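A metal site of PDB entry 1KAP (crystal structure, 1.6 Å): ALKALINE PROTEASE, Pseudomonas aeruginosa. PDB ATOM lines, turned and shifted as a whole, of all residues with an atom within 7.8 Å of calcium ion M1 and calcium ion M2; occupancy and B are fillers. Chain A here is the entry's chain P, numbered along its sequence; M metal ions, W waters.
The side-chain carboxylate (OD2) of Asp 294 sits close to the side-chain hydroxyl (OH) of Tyr 268 (2.6 Å). N of Thr 300 lies within hydrogen-bond range of O of Thr 266 (2.9 Å). The backbone NH (N) of Thr 266 lies within hydrogen-bond range of the backbone carbonyl oxygen (O) of Asn 298, at 3.5 Å. O of Asp 299 sits at hydrogen-bond distance from N of Asn 339. The backbone NH of Gly 297 lies within hydrogen-bond range of the backbone carbonyl oxygen of Thr 263, at 3.4 Å. The guanidinium group (NE) of Arg 262 lies within hydrogen-bond range of the side-chain hydroxyl (OH) of Tyr 268. O of Trp 293 lies within hydrogen-bond range of NH2 of Arg 262, 2.9 Å away.
Within 4 Å of calcium ion M1: Arg 262, Gly 264, Thr 266, Asp 294, Gly 296 and Asp 299. The nearest printed residue that does not touch calcium ion M1 is Thr 263 (4.1 Å).
Of the 24 residues printed, 4 come within 4 Å of calcium ion M2. The nearest printed residue that does not touch calcium ion M2 is Gly 296 (4.2 Å).
Calcium ion M1 is bound by OD1 of Asp 299, O of Gly 296, O of Arg 262, O of Gly 264, OG1 of Thr 266, OD2 of Asp 294 and OD1 of Asp 294. Calcium ion M1 has seven donor atoms within binding distance.
Calcium ion M2 is bound by OD2 of Asp 299 (2.4 Å), O of Gly 297 (2.4 Å), O of Thr 336 (2.4 Å), water W2 (2.4 Å), water W1 (2.4 Å), OE2 of Glu 338 (2.5 Å) and OE1 of Glu 338 (2.5 Å). Calcium ion M2 has seven donor atoms within binding distance.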
ATOM      1  N   THR A 261      -9.035  -6.181 -11.212  1.00  0.00           N
ATOM      2  CA  THR A 261      -8.557  -7.499 -10.806  1.00  0.00           C
ATOM      3  C   THR A 261      -7.834  -8.299 -11.892  1.00  0.00           C
ATOM      4  O   THR A 261      -8.382  -8.508 -12.976  1.00  0.00           O
ATOM      5  CB  THR A 261      -9.729  -8.323 -10.249  1.00  0.00           C
ATOM      6  OG1 THR A 261     -10.264  -7.625  -9.117  1.00  0.00           O
ATOM      7  CG2 THR A 261      -9.276  -9.721  -9.830  1.00  0.00           C
ATOM      8  N   ARG A 262      -6.613  -8.722 -11.593  1.00  0.00           N
ATOM      9  CA  ARG A 262      -5.799  -9.530 -12.505  1.00  0.00           C
ATOM     10  C   ARG A 262      -5.722  -8.958 -13.911  1.00  0.00           C
ATOM     11  O   ARG A 262      -5.949  -9.655 -14.897  1.00  0.00           O
ATOM     12  CB  ARG A 262      -6.329 -10.985 -12.523  1.00  0.00           C
ATOM     13  CG  ARG A 262      -6.090 -11.729 -11.192  1.00  0.00           C
ATOM     14  CD  ARG A 262      -6.713 -13.139 -11.130  1.00  0.00           C
ATOM     15  NE  ARG A 262      -8.177 -13.123 -11.066  1.00  0.00           N
ATOM     16  CZ  ARG A 262      -8.882 -13.066  -9.934  1.00  0.00           C
ATOM     17  NH1 ARG A 262      -8.276 -13.002  -8.753  1.00  0.00           N
ATOM     18  NH2 ARG A 262     -10.217 -13.114  -9.979  1.00  0.00           N
ATOM     19  N   THR A 263      -5.428  -7.652 -14.014  1.00  0.00           N
ATOM     20  CA  THR A 263      -5.330  -6.995 -15.320  1.00  0.00           C
ATOM     21  C   THR A 263      -4.062  -7.360 -16.099  1.00  0.00           C
ATOM     22  O   THR A 263      -3.940  -7.002 -17.263  1.00  0.00           O
ATOM     23  CB  THR A 263      -5.445  -5.436 -15.230  1.00  0.00           C
ATOM     24  OG1 THR A 263      -4.502  -4.923 -14.287  1.00  0.00           O
ATOM     25  CG2 THR A 263      -6.833  -5.029 -14.866  1.00  0.00           C
ATOM     26  N   GLY A 264      -3.108  -8.017 -15.444  1.00  0.00           N
ATOM     27  CA  GLY A 264      -1.897  -8.439 -16.146  1.00  0.00           C
ATOM     28  C   GLY A 264      -2.163  -9.747 -16.885  1.00  0.00           C
ATOM     29  O   GLY A 264      -3.301 -10.204 -16.945  1.00  0.00           O
ATOM     30  N   ASP A 265      -1.136 -10.347 -17.465  1.00  0.00           N
ATOM     31  CA  ASP A 265      -1.294 -11.619 -18.187  1.00  0.00           C
ATOM     32  C   ASP A 265      -1.394 -12.663 -17.094  1.00  0.00           C
ATOM     33  O   ASP A 265      -0.463 -12.849 -16.312  1.00  0.00           O
ATOM     34  CB  ASP A 265      -0.097 -11.884 -19.097  1.00  0.00           C
ATOM     35  CG  ASP A 265       0.068 -10.817 -20.186  1.00  0.00           C
ATOM     36  OD1 ASP A 265      -0.881 -10.055 -20.461  1.00  0.00           O
ATOM     37  OD2 ASP A 265       1.156 -10.742 -20.764  1.00  0.00           O
ATOM     38  N   THR A 266      -2.503 -13.396 -17.077  1.00  0.00           N
ATOM     39  CA  THR A 266      -2.756 -14.337 -15.988  1.00  0.00           C
ATOM     40  C   THR A 266      -2.901 -15.780 -16.412  1.00  0.00           C
ATOM     41  O   THR A 266      -3.545 -16.073 -17.410  1.00  0.00           O
ATOM     42  CB  THR A 266      -4.082 -13.918 -15.269  1.00  0.00           C
ATOM     43  OG1 THR A 266      -4.146 -12.493 -15.154  1.00  0.00           O
ATOM     44  CG2 THR A 266      -4.163 -14.552 -13.883  1.00  0.00           C
ATOM     45  N   VAL A 267      -2.339 -16.685 -15.608  1.00  0.00           N
ATOM     46  CA  VAL A 267      -2.442 -18.119 -15.850  1.00  0.00           C
ATOM     47  C   VAL A 267      -3.262 -18.754 -14.728  1.00  0.00           C
ATOM     48  O   VAL A 267      -3.003 -18.537 -13.536  1.00  0.00           O
ATOM     49  CB  VAL A 267      -1.054 -18.803 -15.854  1.00  0.00           C
ATOM     50  CG1 VAL A 267      -1.210 -20.299 -16.085  1.00  0.00           C
ATOM     51  CG2 VAL A 267      -0.169 -18.179 -16.919  1.00  0.00           C
ATOM     52  N   TYR A 268      -4.284 -19.508 -15.122  1.00  0.00           N
ATOM     53  CA  TYR A 268      -5.169 -20.218 -14.215  1.00  0.00           C
ATOM     54  C   TYR A 268      -4.889 -21.708 -14.357  1.00  0.00           C
ATOM     55  O   TYR A 268      -4.666 -22.198 -15.475  1.00  0.00           O
ATOM     56  CB  TYR A 268      -6.631 -19.953 -14.568  1.00  0.00           C
ATOM     57  CG  TYR A 268      -7.040 -18.506 -14.421  1.00  0.00           C
ATOM     58  CD1 TYR A 268      -6.852 -17.589 -15.468  1.00  0.00           C
ATOM     59  CD2 TYR A 268      -7.536 -18.022 -13.200  1.00  0.00           C
ATOM     60  CE1 TYR A 268      -7.146 -16.221 -15.312  1.00  0.00           C
ATOM     61  CE2 TYR A 268      -7.847 -16.663 -13.031  1.00  0.00           C
ATOM     62  CZ  TYR A 268      -7.638 -15.773 -14.092  1.00  0.00           C
ATOM     63  OH  TYR A 268      -7.878 -14.434 -13.910  1.00  0.00           O
ATOM     64  N   ASN A 273      -0.321 -17.757 -11.587  1.00  0.00           N
ATOM     65  CA  ASN A 273       0.281 -16.545 -11.018  1.00  0.00           C
ATOM     66  C   ASN A 273      -0.841 -15.718 -10.386  1.00  0.00           C
ATOM     67  O   ASN A 273      -0.696 -14.515 -10.203  1.00  0.00           O
ATOM     68  CB  ASN A 273       1.070 -15.732 -12.069  1.00  0.00           C
ATOM     69  CG  ASN A 273       0.182 -15.189 -13.180  1.00  0.00           C
ATOM     70  OD1 ASN A 273      -0.928 -15.657 -13.386  1.00  0.00           O
ATOM     71  ND2 ASN A 273       0.673 -14.185 -13.882  1.00  0.00           N
ATOM     72  N   VAL A 292     -13.776 -18.062 -13.665  1.00  0.00           N
ATOM     73  CA  VAL A 292     -12.776 -17.027 -13.905  1.00  0.00           C
ATOM     74  C   VAL A 292     -13.294 -15.597 -14.013  1.00  0.00           C
ATOM     75  O   VAL A 292     -14.163 -15.315 -14.843  1.00  0.00           O
ATOM     76  CB  VAL A 292     -11.964 -17.339 -15.211  1.00  0.00           C
ATOM     77  CG1 VAL A 292     -10.921 -16.235 -15.500  1.00  0.00           C
ATOM     78  CG2 VAL A 292     -11.320 -18.722 -15.133  1.00  0.00           C
ATOM     79  N   TRP A 293     -12.795 -14.721 -13.147  1.00  0.00           N
ATOM     80  CA  TRP A 293     -13.108 -13.289 -13.246  1.00  0.00           C
ATOM     81  C   TRP A 293     -11.728 -12.700 -13.520  1.00  0.00           C
ATOM     82  O   TRP A 293     -10.786 -12.940 -12.771  1.00  0.00           O
ATOM     83  CB  TRP A 293     -13.697 -12.656 -11.979  1.00  0.00           C
ATOM     84  CG  TRP A 293     -13.807 -11.170 -12.145  1.00  0.00           C
ATOM     85  CD1 TRP A 293     -13.030 -10.215 -11.543  1.00  0.00           C
ATOM     86  CD2 TRP A 293     -14.602 -10.464 -13.119  1.00  0.00           C
ATOM     87  NE1 TRP A 293     -13.273  -8.984 -12.094  1.00  0.00           N
ATOM     88  CE2 TRP A 293     -14.227  -9.100 -13.058  1.00  0.00           C
ATOM     89  CE3 TRP A 293     -15.584 -10.871 -14.038  1.00  0.00           C
ATOM     90  CZ2 TRP A 293     -14.802  -8.125 -13.896  1.00  0.00           C
ATOM     91  CZ3 TRP A 293     -16.155  -9.895 -14.885  1.00  0.00           C
ATOM     92  CH2 TRP A 293     -15.754  -8.543 -14.799  1.00  0.00           C
ATOM     93  N   ASP A 294     -11.604 -11.945 -14.607  1.00  0.00           N
ATOM     94  CA  ASP A 294     -10.311 -11.383 -15.012  1.00  0.00           C
ATOM     95  C   ASP A 294     -10.638 -10.120 -15.810  1.00  0.00           C
ATOM     96  O   ASP A 294     -11.459 -10.159 -16.717  1.00  0.00           O
ATOM     97  CB  ASP A 294      -9.569 -12.423 -15.873  1.00  0.00           C
ATOM     98  CG  ASP A 294      -8.150 -12.000 -16.201  1.00  0.00           C
ATOM     99  OD1 ASP A 294      -7.996 -10.977 -16.901  1.00  0.00           O
ATOM    100  OD2 ASP A 294      -7.209 -12.696 -15.775  1.00  0.00           O
ATOM    101  N   ALA A 295     -10.007  -9.012 -15.443  1.00  0.00           N
ATOM    102  CA  ALA A 295     -10.299  -7.724 -16.071  1.00  0.00           C
ATOM    103  C   ALA A 295      -9.441  -7.283 -17.250  1.00  0.00           C
ATOM    104  O   ALA A 295      -9.697  -6.239 -17.839  1.00  0.00           O
ATOM    105  CB  ALA A 295     -10.319  -6.624 -15.007  1.00  0.00           C
ATOM    106  N   GLY A 296      -8.395  -8.039 -17.585  1.00  0.00           N
ATOM    107  CA  GLY A 296      -7.574  -7.652 -18.721  1.00  0.00           C
ATOM    108  C   GLY A 296      -6.330  -8.484 -18.899  1.00  0.00           C
ATOM    109  O   GLY A 296      -6.037  -9.326 -18.075  1.00  0.00           O
ATOM    110  N   GLY A 297      -5.598  -8.263 -19.987  1.00  0.00           N
ATOM    111  CA  GLY A 297      -4.368  -8.993 -20.219  1.00  0.00           C
ATOM    112  C   GLY A 297      -4.536 -10.225 -21.080  1.00  0.00           C
ATOM    113  O   GLY A 297      -5.645 -10.563 -21.500  1.00  0.00           O
ATOM    114  N   ASN A 298      -3.418 -10.867 -21.386  1.00  0.00           N
ATOM    115  CA  ASN A 298      -3.370 -12.089 -22.197  1.00  0.00           C
ATOM    116  C   ASN A 298      -3.351 -13.226 -21.198  1.00  0.00           C
ATOM    117  O   ASN A 298      -2.343 -13.466 -20.528  1.00  0.00           O
ATOM    118  CB  ASN A 298      -2.105 -12.085 -23.064  1.00  0.00           C
ATOM    119  CG  ASN A 298      -2.027 -13.311 -23.963  1.00  0.00           C
ATOM    120  OD1 ASN A 298      -2.984 -13.643 -24.654  1.00  0.00           O
ATOM    121  ND2 ASN A 298      -0.892 -13.985 -23.943  1.00  0.00           N
ATOM    122  N   ASP A 299      -4.449 -13.952 -21.139  1.00  0.00           N
ATOM    123  CA  ASP A 299      -4.655 -15.004 -20.151  1.00  0.00           C
ATOM    124  C   ASP A 299      -4.702 -16.430 -20.681  1.00  0.00           C
ATOM    125  O   ASP A 299      -5.162 -16.674 -21.802  1.00  0.00           O
ATOM    126  CB  ASP A 299      -5.925 -14.680 -19.378  1.00  0.00           C
ATOM    127  CG  ASP A 299      -6.001 -13.212 -19.002  1.00  0.00           C
ATOM    128  OD1 ASP A 299      -5.099 -12.754 -18.269  1.00  0.00           O
ATOM    129  OD2 ASP A 299      -6.907 -12.513 -19.465  1.00  0.00           O
ATOM    130  N   THR A 300      -4.360 -17.367 -19.817  1.00  0.00           N
ATOM    131  CA  THR A 300      -4.271 -18.763 -20.201  1.00  0.00           C
ATOM    132  C   THR A 300      -4.854 -19.727 -19.179  1.00  0.00           C
ATOM    133  O   THR A 300      -4.653 -19.559 -17.967  1.00  0.00           O
ATOM    134  CB  THR A 300      -2.766 -19.157 -20.340  1.00  0.00           C
ATOM    135  OG1 THR A 300      -2.132 -18.290 -21.299  1.00  0.00           O
ATOM    136  CG2 THR A 300      -2.597 -20.623 -20.768  1.00  0.00           C
ATOM    137  N   VAL A 335     -15.829 -11.701 -19.571  1.00  0.00           N
ATOM    138  CA  VAL A 335     -14.416 -11.996 -19.453  1.00  0.00           C
ATOM    139  C   VAL A 335     -13.862 -12.633 -20.728  1.00  0.00           C
ATOM    140  O   VAL A 335     -14.475 -13.553 -21.283  1.00  0.00           O
ATOM    141  CB  VAL A 335     -14.163 -12.956 -18.274  1.00  0.00           C
ATOM    142  CG1 VAL A 335     -12.706 -13.417 -18.263  1.00  0.00           C
ATOM    143  CG2 VAL A 335     -14.519 -12.254 -16.976  1.00  0.00           C
ATOM    144  N   THR A 336     -12.713 -12.142 -21.183  1.00  0.00           N
ATOM    145  CA  THR A 336     -12.076 -12.703 -22.370  1.00  0.00           C
ATOM    146  C   THR A 336     -10.780 -13.419 -21.994  1.00  0.00           C
ATOM    147  O   THR A 336      -9.811 -12.787 -21.573  1.00  0.00           O
ATOM    148  CB  THR A 336     -11.777 -11.627 -23.466  1.00  0.00           C
ATOM    149  OG1 THR A 336     -13.000 -10.949 -23.807  1.00  0.00           O
ATOM    150  CG2 THR A 336     -11.175 -12.262 -24.726  1.00  0.00           C
ATOM    151  N   VAL A 337     -10.804 -14.740 -22.100  1.00  0.00           N
ATOM    152  CA  VAL A 337      -9.632 -15.584 -21.839  1.00  0.00           C
ATOM    153  C   VAL A 337      -9.127 -15.986 -23.241  1.00  0.00           C
ATOM    154  O   VAL A 337      -9.909 -16.451 -24.080  1.00  0.00           O
ATOM    155  CB  VAL A 337      -9.990 -16.802 -20.985  1.00  0.00           C
ATOM    156  CG1 VAL A 337      -8.747 -17.676 -20.791  1.00  0.00           C
ATOM    157  CG2 VAL A 337     -10.515 -16.321 -19.619  1.00  0.00           C
ATOM    158  N   GLU A 338      -7.830 -15.824 -23.446  1.00  0.00           N
ATOM    159  CA  GLU A 338      -7.235 -16.029 -24.756  1.00  0.00           C
ATOM    160  C   GLU A 338      -6.666 -17.374 -25.137  1.00  0.00           C
ATOM    161  O   GLU A 338      -6.799 -17.805 -26.283  1.00  0.00           O
ATOM    162  CB  GLU A 338      -6.141 -14.973 -24.988  1.00  0.00           C
ATOM    163  CG  GLU A 338      -6.612 -13.523 -25.102  1.00  0.00           C
ATOM    164  CD  GLU A 338      -7.055 -12.869 -23.788  1.00  0.00           C
ATOM    165  OE1 GLU A 338      -6.772 -13.392 -22.684  1.00  0.00           O
ATOM    166  OE2 GLU A 338      -7.693 -11.801 -23.862  1.00  0.00           O
ATOM    167  N   ASN A 339      -6.024 -18.047 -24.185  1.00  0.00           N
ATOM    168  CA  ASN A 339      -5.331 -19.293 -24.500  1.00  0.00           C
ATOM    169  C   ASN A 339      -5.717 -20.457 -23.610  1.00  0.00           C
ATOM    170  O   ASN A 339      -6.211 -20.265 -22.509  1.00  0.00           O
ATOM    171  CB  ASN A 339      -3.817 -19.041 -24.349  1.00  0.00           C
ATOM    172  CG  ASN A 339      -3.405 -17.718 -24.946  1.00  0.00           C
ATOM    173  OD1 ASN A 339      -3.681 -17.438 -26.106  1.00  0.00           O
ATOM    174  ND2 ASN A 339      -2.802 -16.855 -24.128  1.00  0.00           N
ATOM    175  N   VAL A 354     -11.773 -14.246 -30.402  1.00  0.00           N
ATOM    176  CA  VAL A 354     -10.509 -13.544 -30.567  1.00  0.00           C
ATOM    177  C   VAL A 354      -9.410 -14.515 -30.976  1.00  0.00           C
ATOM    178  O   VAL A 354      -9.640 -15.722 -31.045  1.00  0.00           O
ATOM    179  CB  VAL A 354     -10.087 -12.750 -29.272  1.00  0.00           C
ATOM    180  CG1 VAL A 354     -11.216 -11.791 -28.870  1.00  0.00           C
ATOM    181  CG2 VAL A 354      -9.720 -13.693 -28.109  1.00  0.00           C
HETATM  182 CA    CA M   1      -5.522 -11.130 -16.683  1.00  0.00          CA
HETATM  183 CA    CA M   2      -7.826 -11.488 -21.376  1.00  0.00          CA
HETATM  184  O   HOH W   1      -8.977 -10.572 -19.436  1.00  0.00           O
HETATM  185  O   HOH W   2      -8.701  -9.413 -22.249  1.00  0.00           O
